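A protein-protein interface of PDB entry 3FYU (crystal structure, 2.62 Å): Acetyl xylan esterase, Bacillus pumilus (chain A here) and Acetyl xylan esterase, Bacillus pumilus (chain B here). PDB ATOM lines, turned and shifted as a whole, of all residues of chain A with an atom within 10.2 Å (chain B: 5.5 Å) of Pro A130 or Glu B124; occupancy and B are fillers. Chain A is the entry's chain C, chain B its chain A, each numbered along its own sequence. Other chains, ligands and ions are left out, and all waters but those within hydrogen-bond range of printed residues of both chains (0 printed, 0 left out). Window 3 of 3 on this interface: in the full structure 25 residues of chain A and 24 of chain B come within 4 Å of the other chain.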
ATOM      1  N   ASP A 125      11.094   9.828  15.856  1.00  0.00           N
ATOM      2  CA  ASP A 125      10.707  10.232  14.513  1.00  0.00           C
ATOM      3  C   ASP A 125       9.435   9.458  14.171  1.00  0.00           C
ATOM      4  O   ASP A 125       9.490   8.267  13.859  1.00  0.00           O
ATOM      5  CB  ASP A 125      11.798   9.913  13.498  1.00  0.00           C
ATOM      6  CG  ASP A 125      11.461  10.441  12.115  1.00  0.00           C
ATOM      7  OD1 ASP A 125      10.309  10.889  11.929  1.00  0.00           O
ATOM      8  OD2 ASP A 125      12.329  10.413  11.214  1.00  0.00           O
ATOM      9  N   THR A 126       8.288  10.126  14.247  1.00  0.00           N
ATOM     10  CA  THR A 126       7.017   9.459  13.953  1.00  0.00           C
ATOM     11  C   THR A 126       6.752   9.373  12.460  1.00  0.00           C
ATOM     12  O   THR A 126       5.882   8.627  12.032  1.00  0.00           O
ATOM     13  CB  THR A 126       5.826  10.183  14.584  1.00  0.00           C
ATOM     14  OG1 THR A 126       5.804  11.529  14.109  1.00  0.00           O
ATOM     15  CG2 THR A 126       5.925  10.177  16.090  1.00  0.00           C
ATOM     16  N   SER A 127       7.501  10.128  11.671  1.00  0.00           N
ATOM     17  CA  SER A 127       7.277  10.108  10.248  1.00  0.00           C
ATOM     18  C   SER A 127       7.528   8.721   9.683  1.00  0.00           C
ATOM     19  O   SER A 127       8.553   8.088   9.944  1.00  0.00           O
ATOM     20  CB  SER A 127       8.146  11.151   9.544  1.00  0.00           C
ATOM     21  OG  SER A 127       9.506  10.802   9.598  1.00  0.00           O
ATOM     22  N   VAL A 128       6.550   8.262   8.912  1.00  0.00           N
ATOM     23  CA  VAL A 128       6.555   6.965   8.257  1.00  0.00           C
ATOM     24  C   VAL A 128       7.579   6.900   7.127  1.00  0.00           C
ATOM     25  O   VAL A 128       7.958   7.919   6.562  1.00  0.00           O
ATOM     26  CB  VAL A 128       5.136   6.686   7.679  1.00  0.00           C
ATOM     27  CG1 VAL A 128       5.136   5.459   6.790  1.00  0.00           C
ATOM     28  CG2 VAL A 128       4.149   6.512   8.820  1.00  0.00           C
ATOM     29  N   THR A 129       8.032   5.695   6.809  1.00  0.00           N
ATOM     30  CA  THR A 129       8.962   5.499   5.705  1.00  0.00           C
ATOM     31  C   THR A 129       8.071   5.118   4.520  1.00  0.00           C
ATOM     32  O   THR A 129       7.568   3.998   4.445  1.00  0.00           O
ATOM     33  CB  THR A 129       9.948   4.348   5.983  1.00  0.00           C
ATOM     34  OG1 THR A 129      10.672   4.618   7.191  1.00  0.00           O
ATOM     35  CG2 THR A 129      10.927   4.198   4.816  1.00  0.00           C
ATOM     36  N   PRO A 130       7.841   6.059   3.595  1.00  0.00           N
ATOM     37  CA  PRO A 130       7.004   5.819   2.422  1.00  0.00           C
ATOM     38  C   PRO A 130       7.428   4.585   1.632  1.00  0.00           C
ATOM     39  O   PRO A 130       6.596   3.760   1.251  1.00  0.00           O
ATOM     40  CB  PRO A 130       7.168   7.109   1.612  1.00  0.00           C
ATOM     41  CG  PRO A 130       7.440   8.142   2.659  1.00  0.00           C
ATOM     42  CD  PRO A 130       8.402   7.419   3.566  1.00  0.00           C
ATOM     43  N   GLY A 131       8.726   4.457   1.385  1.00  0.00           N
ATOM     44  CA  GLY A 131       9.198   3.322   0.618  1.00  0.00           C
ATOM     45  C   GLY A 131      10.683   3.072   0.734  1.00  0.00           C
ATOM     46  O   GLY A 131      11.335   3.525   1.670  1.00  0.00           O
ATOM     47  N   GLY A 132      11.219   2.348  -0.237  1.00  0.00           N
ATOM     48  CA  GLY A 132      12.627   2.026  -0.217  1.00  0.00           C
ATOM     49  C   GLY A 132      13.523   3.238  -0.304  1.00  0.00           C
ATOM     50  O   GLY A 132      13.166   4.241  -0.911  1.00  0.00           O
ATOM     51  N   HIS A 133      14.690   3.132   0.320  1.00  0.00           N
ATOM     52  CA  HIS A 133      15.672   4.196   0.299  1.00  0.00           C
ATOM     53  C   HIS A 133      17.039   3.627   0.665  1.00  0.00           C
ATOM     54  O   HIS A 133      17.142   2.523   1.210  1.00  0.00           O
ATOM     55  CB  HIS A 133      15.257   5.331   1.253  1.00  0.00           C
ATOM     56  CG  HIS A 133      15.234   4.952   2.702  1.00  0.00           C
ATOM     57  ND1 HIS A 133      16.374   4.872   3.471  1.00  0.00           N
ATOM     58  CD2 HIS A 133      14.201   4.688   3.537  1.00  0.00           C
ATOM     59  CE1 HIS A 133      16.045   4.582   4.717  1.00  0.00           C
ATOM     60  NE2 HIS A 133      14.732   4.466   4.785  1.00  0.00           N
ATOM     61  N   TRP A 137      19.643   8.144   6.546  1.00  0.00           N
ATOM     62  CA  TRP A 137      18.500   9.047   6.647  1.00  0.00           C
ATOM     63  C   TRP A 137      18.409   9.984   5.448  1.00  0.00           C
ATOM     64  O   TRP A 137      17.351  10.529   5.164  1.00  0.00           O
ATOM     65  CB  TRP A 137      18.608   9.896   7.912  1.00  0.00           C
ATOM     66  CG  TRP A 137      18.520   9.125   9.181  1.00  0.00           C
ATOM     67  CD1 TRP A 137      17.381   8.744   9.827  1.00  0.00           C
ATOM     68  CD2 TRP A 137      19.617   8.652   9.981  1.00  0.00           C
ATOM     69  NE1 TRP A 137      17.695   8.070  10.984  1.00  0.00           N
ATOM     70  CE2 TRP A 137      19.060   7.999  11.102  1.00  0.00           C
ATOM     71  CE3 TRP A 137      21.014   8.721   9.862  1.00  0.00           C
ATOM     72  CZ2 TRP A 137      19.852   7.419  12.099  1.00  0.00           C
ATOM     73  CZ3 TRP A 137      21.799   8.148  10.852  1.00  0.00           C
ATOM     74  CH2 TRP A 137      21.215   7.507  11.955  1.00  0.00           C
ATOM     75  N   THR A 139      17.984   9.677   2.319  1.00  0.00           N
ATOM     76  CA  THR A 139      16.973   9.477   1.300  1.00  0.00           C
ATOM     77  C   THR A 139      15.643   8.999   1.835  1.00  0.00           C
ATOM     78  O   THR A 139      14.779   8.598   1.066  1.00  0.00           O
ATOM     79  CB  THR A 139      17.467   8.481   0.223  1.00  0.00           C
ATOM     80  OG1 THR A 139      17.810   7.235   0.839  1.00  0.00           O
ATOM     81  CG2 THR A 139      18.689   9.032  -0.491  1.00  0.00           C
ATOM     82  N   LYS A 140      15.467   9.035   3.152  1.00  0.00           N
ATOM     83  CA  LYS A 140      14.204   8.587   3.737  1.00  0.00           C
ATOM     84  C   LYS A 140      13.078   9.548   3.338  1.00  0.00           C
ATOM     85  O   LYS A 140      13.128  10.744   3.645  1.00  0.00           O
ATOM     86  CB  LYS A 140      14.298   8.518   5.266  1.00  0.00           C
ATOM     87  CG  LYS A 140      13.049   7.943   5.907  1.00  0.00           C
ATOM     88  CD  LYS A 140      13.059   8.079   7.421  1.00  0.00           C
ATOM     89  CE  LYS A 140      11.707   7.668   8.011  1.00  0.00           C
ATOM     90  NZ  LYS A 140      11.497   8.134   9.418  1.00  0.00           N
ATOM     91  N   GLY A 141      12.076   9.017   2.639  1.00  0.00           N
ATOM     92  CA  GLY A 141      10.952   9.824   2.202  1.00  0.00           C
ATOM     93  C   GLY A 141      11.330  10.866   1.169  1.00  0.00           C
ATOM     94  O   GLY A 141      10.625  11.857   0.997  1.00  0.00           O
ATOM     95  N   ILE A 142      12.427  10.631   0.465  1.00  0.00           N
ATOM     96  CA  ILE A 142      12.919  11.577  -0.531  1.00  0.00           C
ATOM     97  C   ILE A 142      12.032  11.841  -1.758  1.00  0.00           C
ATOM     98  O   ILE A 142      12.268  12.804  -2.485  1.00  0.00           O
ATOM     99  CB  ILE A 142      14.334  11.166  -1.038  1.00  0.00           C
ATOM    100  CG1 ILE A 142      15.004  12.352  -1.719  1.00  0.00           C
ATOM    101  CG2 ILE A 142      14.239  10.014  -2.034  1.00  0.00           C
ATOM    102  CD1 ILE A 142      16.470  12.182  -1.892  1.00  0.00           C
ATOM    103  N   LEU A 143      11.022  11.007  -1.998  1.00  0.00           N
ATOM    104  CA  LEU A 143      10.165  11.214  -3.165  1.00  0.00           C
ATOM    105  C   LEU A 143       9.075  12.265  -2.972  1.00  0.00           C
ATOM    106  O   LEU A 143       8.213  12.439  -3.833  1.00  0.00           O
ATOM    107  CB  LEU A 143       9.547   9.889  -3.605  1.00  0.00           C
ATOM    108  CG  LEU A 143      10.583   8.960  -4.248  1.00  0.00           C
ATOM    109  CD1 LEU A 143       9.904   7.723  -4.794  1.00  0.00           C
ATOM    110  CD2 LEU A 143      11.317   9.697  -5.363  1.00  0.00           C
ATOM    111  N   SER A 144       9.122  12.972  -1.850  1.00  0.00           N
ATOM    112  CA  SER A 144       8.144  14.008  -1.577  1.00  0.00           C
ATOM    113  C   SER A 144       8.591  14.928  -0.454  1.00  0.00           C
ATOM    114  O   SER A 144       9.001  14.470   0.608  1.00  0.00           O
ATOM    115  CB  SER A 144       6.794  13.379  -1.216  1.00  0.00           C
ATOM    116  OG  SER A 144       5.850  14.372  -0.848  1.00  0.00           O
ATOM    117  N   LYS A 145       8.494  16.228  -0.689  1.00  0.00           N
ATOM    118  CA  LYS A 145       8.885  17.211   0.310  1.00  0.00           C
ATOM    119  C   LYS A 145       8.100  17.060   1.608  1.00  0.00           C
ATOM    120  O   LYS A 145       8.581  17.442   2.669  1.00  0.00           O
ATOM    121  CB  LYS A 145       8.702  18.622  -0.243  1.00  0.00           C
ATOM    122  CG  LYS A 145       7.282  18.945  -0.708  1.00  0.00           C
ATOM    123  CD  LYS A 145       7.220  20.344  -1.308  1.00  0.00           C
ATOM    124  CE  LYS A 145       5.822  20.708  -1.769  1.00  0.00           C
ATOM    125  NZ  LYS A 145       5.345  19.798  -2.827  1.00  0.00           N
ATOM    126  N   ASP A 146       6.897  16.496   1.531  1.00  0.00           N
ATOM    127  CA  ASP A 146       6.085  16.329   2.733  1.00  0.00           C
ATOM    128  C   ASP A 146       6.574  15.186   3.598  1.00  0.00           C
ATOM    129  O   ASP A 146       6.443  15.218   4.817  1.00  0.00           O
ATOM    130  CB  ASP A 146       4.612  16.080   2.381  1.00  0.00           C
ATOM    131  CG  ASP A 146       3.942  17.294   1.775  1.00  0.00           C
ATOM    132  OD1 ASP A 146       4.311  18.427   2.168  1.00  0.00           O
ATOM    133  OD2 ASP A 146       3.042  17.117   0.919  1.00  0.00           O
ATOM    134  N   THR A 147       7.145  14.175   2.959  1.00  0.00           N
ATOM    135  CA  THR A 147       7.618  12.996   3.675  1.00  0.00           C
ATOM    136  C   THR A 147       9.118  12.993   3.960  1.00  0.00           C
ATOM    137  O   THR A 147       9.593  12.180   4.748  1.00  0.00           O
ATOM    138  CB  THR A 147       7.298  11.722   2.878  1.00  0.00           C
ATOM    139  OG1 THR A 147       7.947  11.797   1.603  1.00  0.00           O
ATOM    140  CG2 THR A 147       5.800  11.579   2.674  1.00  0.00           C
ATOM    141  N   TYR A 148       9.859  13.897   3.332  1.00  0.00           N
ATOM    142  CA  TYR A 148      11.300  13.920   3.512  1.00  0.00           C
ATOM    143  C   TYR A 148      11.791  14.049   4.962  1.00  0.00           C
ATOM    144  O   TYR A 148      11.307  14.878   5.745  1.00  0.00           O
ATOM    145  CB  TYR A 148      11.922  15.009   2.641  1.00  0.00           C
ATOM    146  CG  TYR A 148      13.419  14.902   2.555  1.00  0.00           C
ATOM    147  CD1 TYR A 148      14.023  13.707   2.169  1.00  0.00           C
ATOM    148  CD2 TYR A 148      14.234  15.979   2.882  1.00  0.00           C
ATOM    149  CE1 TYR A 148      15.399  13.583   2.119  1.00  0.00           C
ATOM    150  CE2 TYR A 148      15.619  15.868   2.832  1.00  0.00           C
ATOM    151  CZ  TYR A 148      16.193  14.662   2.449  1.00  0.00           C
ATOM    152  OH  TYR A 148      17.561  14.541   2.383  1.00  0.00           O
ATOM    153  N   TYR A 149      12.770  13.213   5.295  1.00  0.00           N
ATOM    154  CA  TYR A 149      13.353  13.154   6.623  1.00  0.00           C
ATOM    155  C   TYR A 149      13.617  14.495   7.287  1.00  0.00           C
ATOM    156  O   TYR A 149      13.218  14.716   8.427  1.00  0.00           O
ATOM    157  CB  TYR A 149      14.656  12.356   6.578  1.00  0.00           C
ATOM    158  CG  TYR A 149      15.404  12.343   7.892  1.00  0.00           C
ATOM    159  CD1 TYR A 149      14.886  11.683   9.005  1.00  0.00           C
ATOM    160  CD2 TYR A 149      16.630  12.995   8.021  1.00  0.00           C
ATOM    161  CE1 TYR A 149      15.574  11.669  10.216  1.00  0.00           C
ATOM    162  CE2 TYR A 149      17.326  12.989   9.225  1.00  0.00           C
ATOM    163  CZ  TYR A 149      16.799  12.323  10.316  1.00  0.00           C
ATOM    164  OH  TYR A 149      17.507  12.289  11.502  1.00  0.00           O
ATOM    165  N   TYR A 228      21.092   5.716  -3.512  1.00  0.00           N
ATOM    166  CA  TYR A 228      19.653   5.650  -3.710  1.00  0.00           C
ATOM    167  C   TYR A 228      19.320   5.515  -5.196  1.00  0.00           C
ATOM    168  O   TYR A 228      18.525   4.662  -5.581  1.00  0.00           O
ATOM    169  CB  TYR A 228      18.996   6.902  -3.136  1.00  0.00           C
ATOM    170  CG  TYR A 228      17.505   6.974  -3.371  1.00  0.00           C
ATOM    171  CD1 TYR A 228      16.622   6.174  -2.650  1.00  0.00           C
ATOM    172  CD2 TYR A 228      16.978   7.827  -4.342  1.00  0.00           C
ATOM    173  CE1 TYR A 228      15.250   6.223  -2.895  1.00  0.00           C
ATOM    174  CE2 TYR A 228      15.614   7.882  -4.592  1.00  0.00           C
ATOM    175  CZ  TYR A 228      14.757   7.080  -3.868  1.00  0.00           C
ATOM    176  OH  TYR A 228      13.407   7.147  -4.116  1.00  0.00           O
ATOM    177  N   ASN A 232      17.326   2.738  -7.575  1.00  0.00           N
ATOM    178  CA  ASN A 232      16.102   3.120  -8.270  1.00  0.00           C
ATOM    179  C   ASN A 232      16.522   3.835  -9.542  1.00  0.00           C
ATOM    180  O   ASN A 232      16.623   5.063  -9.565  1.00  0.00           O
ATOM    181  CB  ASN A 232      15.252   4.048  -7.418  1.00  0.00           C
ATOM    182  CG  ASN A 232      14.806   3.401  -6.129  1.00  0.00           C
ATOM    183  OD1 ASN A 232      15.583   3.278  -5.175  1.00  0.00           O
ATOM    184  ND2 ASN A 232      13.548   2.976  -6.090  1.00  0.00           N
ATOM    185  N   THR A 244      12.629  17.255  -4.467  1.00  0.00           N
ATOM    186  CA  THR A 244      12.397  17.218  -3.029  1.00  0.00           C
ATOM    187  C   THR A 244      13.510  17.930  -2.266  1.00  0.00           C
ATOM    188  O   THR A 244      13.257  18.822  -1.446  1.00  0.00           O
ATOM    189  CB  THR A 244      12.308  15.777  -2.533  1.00  0.00           C
ATOM    190  OG1 THR A 244      11.201  15.136  -3.171  1.00  0.00           O
ATOM    191  CG2 THR A 244      12.100  15.736  -1.030  1.00  0.00           C
ATOM    192  N   GLN B  62      -1.259  -5.285   2.562  1.00  0.00           N
ATOM    193  CA  GLN B  62      -1.185  -4.641   3.860  1.00  0.00           C
ATOM    194  C   GLN B  62      -0.659  -5.635   4.879  1.00  0.00           C
ATOM    195  O   GLN B  62      -1.055  -6.801   4.883  1.00  0.00           O
ATOM    196  CB  GLN B  62      -2.574  -4.154   4.260  1.00  0.00           C
ATOM    197  CG  GLN B  62      -3.173  -3.174   3.264  1.00  0.00           C
ATOM    198  CD  GLN B  62      -2.286  -1.958   3.055  1.00  0.00           C
ATOM    199  OE1 GLN B  62      -1.968  -1.245   4.007  1.00  0.00           O
ATOM    200  NE2 GLN B  62      -1.876  -1.720   1.809  1.00  0.00           N
ATOM    201  N   HIS B  66      -0.220  -1.830   9.406  1.00  0.00           N
ATOM    202  CA  HIS B  66      -0.912  -1.309   8.229  1.00  0.00           C
ATOM    203  C   HIS B  66       0.076  -0.763   7.219  1.00  0.00           C
ATOM    204  O   HIS B  66      -0.192   0.230   6.544  1.00  0.00           O
ATOM    205  CB  HIS B  66      -1.902  -0.206   8.640  1.00  0.00           C
ATOM    206  CG  HIS B  66      -3.035  -0.706   9.480  1.00  0.00           C
ATOM    207  ND1 HIS B  66      -4.070  -1.454   8.959  1.00  0.00           N
ATOM    208  CD2 HIS B  66      -3.265  -0.619  10.811  1.00  0.00           C
ATOM    209  CE1 HIS B  66      -4.888  -1.808   9.934  1.00  0.00           C
ATOM    210  NE2 HIS B  66      -4.422  -1.314  11.068  1.00  0.00           N
ATOM    211  N   SER B  67       1.226  -1.410   7.122  1.00  0.00           N
ATOM    212  CA  SER B  67       2.241  -0.984   6.173  1.00  0.00           C
ATOM    213  C   SER B  67       1.940  -1.638   4.832  1.00  0.00           C
ATOM    214  O   SER B  67       1.474  -2.777   4.777  1.00  0.00           O
ATOM    215  CB  SER B  67       3.643  -1.398   6.648  1.00  0.00           C
ATOM    216  OG  SER B  67       3.989  -0.771   7.868  1.00  0.00           O
ATOM    217  N   LYS B  68       2.194  -0.904   3.758  1.00  0.00           N
ATOM    218  CA  LYS B  68       1.951  -1.411   2.426  1.00  0.00           C
ATOM    219  C   LYS B  68       3.246  -2.001   1.903  1.00  0.00           C
ATOM    220  O   LYS B  68       4.198  -1.275   1.610  1.00  0.00           O
ATOM    221  CB  LYS B  68       1.478  -0.281   1.513  1.00  0.00           C
ATOM    222  CG  LYS B  68       1.002  -0.753   0.152  1.00  0.00           C
ATOM    223  CD  LYS B  68       0.339   0.381  -0.614  1.00  0.00           C
ATOM    224  CE  LYS B  68      -0.204  -0.102  -1.948  1.00  0.00           C
ATOM    225  NZ  LYS B  68      -0.799   1.003  -2.742  1.00  0.00           N
ATOM    226  N   ILE B  69       3.269  -3.325   1.790  1.00  0.00           N
ATOM    227  CA  ILE B  69       4.440  -4.054   1.314  1.00  0.00           C
ATOM    228  C   ILE B  69       4.308  -4.313  -0.183  1.00  0.00           C
ATOM    229  O   ILE B  69       3.222  -4.608  -0.666  1.00  0.00           O
ATOM    230  CB  ILE B  69       4.573  -5.398   2.062  1.00  0.00           C
ATOM    231  CG1 ILE B  69       4.488  -5.162   3.571  1.00  0.00           C
ATOM    232  CG2 ILE B  69       5.889  -6.064   1.718  1.00  0.00           C
ATOM    233  CD1 ILE B  69       5.448  -4.122   4.085  1.00  0.00           C
ATOM    234  N   ARG B 118      10.900  -3.520   4.070  1.00  0.00           N
ATOM    235  CA  ARG B 118      10.564  -2.177   4.552  1.00  0.00           C
ATOM    236  C   ARG B 118      11.661  -1.125   4.483  1.00  0.00           C
ATOM    237  O   ARG B 118      12.739  -1.287   5.062  1.00  0.00           O
ATOM    238  CB  ARG B 118      10.094  -2.243   6.000  1.00  0.00           C
ATOM    239  CG  ARG B 118       8.870  -3.076   6.232  1.00  0.00           C
ATOM    240  CD  ARG B 118       8.402  -2.886   7.656  1.00  0.00           C
ATOM    241  NE  ARG B 118       7.200  -3.651   7.914  1.00  0.00           N
ATOM    242  CZ  ARG B 118       6.269  -3.302   8.787  1.00  0.00           C
ATOM    243  NH1 ARG B 118       6.403  -2.190   9.495  1.00  0.00           N
ATOM    244  NH2 ARG B 118       5.195  -4.069   8.936  1.00  0.00           N
ATOM    245  N   GLY B 119      11.372  -0.031   3.789  1.00  0.00           N
ATOM    246  CA  GLY B 119      12.336   1.050   3.691  1.00  0.00           C
ATOM    247  C   GLY B 119      13.643   0.751   2.982  1.00  0.00           C
ATOM    248  O   GLY B 119      14.464   1.653   2.780  1.00  0.00           O
ATOM    249  N   GLY B 122      12.235  -1.379  -0.999  1.00  0.00           N
ATOM    250  CA  GLY B 122      10.911  -0.880  -1.285  1.00  0.00           C
ATOM    251  C   GLY B 122      10.024  -1.095  -0.087  1.00  0.00           C
ATOM    252  O   GLY B 122      10.511  -1.350   1.014  1.00  0.00           O
ATOM    253  N   SER B 123       8.719  -0.981  -0.297  1.00  0.00           N
ATOM    254  CA  SER B 123       7.752  -1.188   0.763  1.00  0.00           C
ATOM    255  C   SER B 123       7.757  -0.074   1.783  1.00  0.00           C
ATOM    256  O   SER B 123       8.765   0.594   1.995  1.00  0.00           O
ATOM    257  CB  SER B 123       8.001  -2.528   1.459  1.00  0.00           C
ATOM    258  OG  SER B 123       7.753  -3.607   0.577  1.00  0.00           O
ATOM    259  N   GLU B 124       6.605   0.102   2.415  1.00  0.00           N
ATOM    260  CA  GLU B 124       6.394   1.135   3.413  1.00  0.00           C
ATOM    261  C   GLU B 124       6.618   0.599   4.825  1.00  0.00           C
ATOM    262  O   GLU B 124       6.280  -0.539   5.122  1.00  0.00           O
ATOM    263  CB  GLU B 124       4.961   1.681   3.281  1.00  0.00           C
ATOM    264  CG  GLU B 124       4.435   2.385   4.534  1.00  0.00           C
ATOM    265  CD  GLU B 124       2.966   2.740   4.442  1.00  0.00           C
ATOM    266  OE1 GLU B 124       2.158   1.831   4.166  1.00  0.00           O
ATOM    267  OE2 GLU B 124       2.624   3.928   4.654  1.00  0.00           O
ATOM    268  N   ASP B 125       7.205   1.420   5.688  1.00  0.00           N
ATOM    269  CA  ASP B 125       7.423   1.027   7.069  1.00  0.00           C
ATOM    270  C   ASP B 125       6.754   2.091   7.915  1.00  0.00           C
ATOM    271  O   ASP B 125       7.279   3.202   8.057  1.00  0.00           O
ATOM    272  CB  ASP B 125       8.913   0.964   7.409  1.00  0.00           C
ATOM    273  CG  ASP B 125       9.161   0.441   8.812  1.00  0.00           C
ATOM    274  OD1 ASP B 125       8.167   0.214   9.531  1.00  0.00           O
ATOM    275  OD2 ASP B 125      10.335   0.259   9.202  1.00  0.00           O
ATOM    276  N   THR B 126       5.585   1.758   8.458  1.00  0.00           N
ATOM    277  CA  THR B 126       4.846   2.701   9.281  1.00  0.00           C
ATOM    278  C   THR B 126       5.344   2.735  10.712  1.00  0.00           C
ATOM    279  O   THR B 126       4.988   3.632  11.474  1.00  0.00           O
ATOM    280  CB  THR B 126       3.350   2.371   9.317  1.00  0.00           C
ATOM    281  OG1 THR B 126       3.152   1.062   9.871  1.00  0.00           O
ATOM    282  CG2 THR B 126       2.769   2.440   7.920  1.00  0.00           C
ATOM    283  N   ASP B 156       5.929  -9.230   7.660  1.00  0.00           N
ATOM    284  CA  ASP B 156       5.659  -8.970   6.250  1.00  0.00           C
ATOM    285  C   ASP B 156       5.947 -10.259   5.469  1.00  0.00           C
ATOM    286  O   ASP B 156       5.240 -10.598   4.521  1.00  0.00           O
ATOM    287  CB  ASP B 156       6.562  -7.859   5.681  1.00  0.00           C
ATOM    288  CG  ASP B 156       6.349  -6.504   6.338  1.00  0.00           C
ATOM    289  OD1 ASP B 156       5.221  -6.171   6.763  1.00  0.00           O
ATOM    290  OD2 ASP B 156       7.334  -5.748   6.400  1.00  0.00           O
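Printed residues of chain B that touch a printed residue of chain A: Gly B119, Gly B122, Ser B123, Glu B124, Asp B125 and Thr B126.
Among the printed residues, no Asp or Glu carboxylate lies within 4 Å of a Lys or Arg side-chain nitrogen of the other chain.
OG of Ser B67 lies within hydrogen-bond range of OG1 of Thr B126 (2.8 Å).
The backbone NH of Lys B68 is in hydrogen-bond range of the side-chain carboxylate of Glu B124 (2.8 Å).
The guanidinium group of Arg B118 lies within salt-bridge range of the side-chain carboxylate of Asp B125 (3.0 Å).
Pro A130 touches two residues of chain B.
Of chain A, only Val A128 (3.6 Å), Thr A129 (3.3 Å) and Pro A130 (3.3 Å) come within 4 Å of Glu B124.
Ser B67 touches none of the printed residues of chain A.
Of chain A, only Pro A130 (3.9 Å), Gly A131 (3.1 Å) and Gly A132 (3.8 Å) come within 4 Å of Ser B123.
Of the printed residues of chain B, Gly A132 touches Gly B119 (3.5 Å), Gly B122 (3.4 Å) and Ser B123 (3.8 Å).
Of the printed residues of chain B, Val A128 touches Glu B124, Asp B125 and Thr B126.
Thr A244 touches none of the printed residues of chain B.
The nearest residue of chain B that does not touch Pro A130 is Asp B125 (5.1 Å).
The nearest printed residue of chain B that does not touch Gly A131 is Gly B122 (4.3 Å).
O of Gly B119 is in hydrogen-bond range of N of His A133 (2.9 Å).
The backbone NH (N) of Asp B125 lies within hydrogen-bond range of the backbone carbonyl oxygen (O) of Thr A129 (2.9 Å).
Among the printed residues, pairs that only touch across the chains: Val A128 with Glu B124 (3.6 Å), Val A128 with Asp B125 (3.4 Å), Val A128 with Thr B126 (3.7 Å), Thr A129 with Gly B119 (3.6 Å), Thr A129 with Glu B124 (3.3 Å), Pro A130 with Ser B123 (3.9 Å), Pro A130 with Glu B124 (3.3 Å), Gly A131 with Gly B119 (3.3 Å), Gly A131 with Ser B123 (3.1 Å), Gly A132 with Gly B119 (3.5 Å), Gly A132 with Gly B122 (3.4 Å) and Gly A132 with Ser B123 (3.8 Å).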
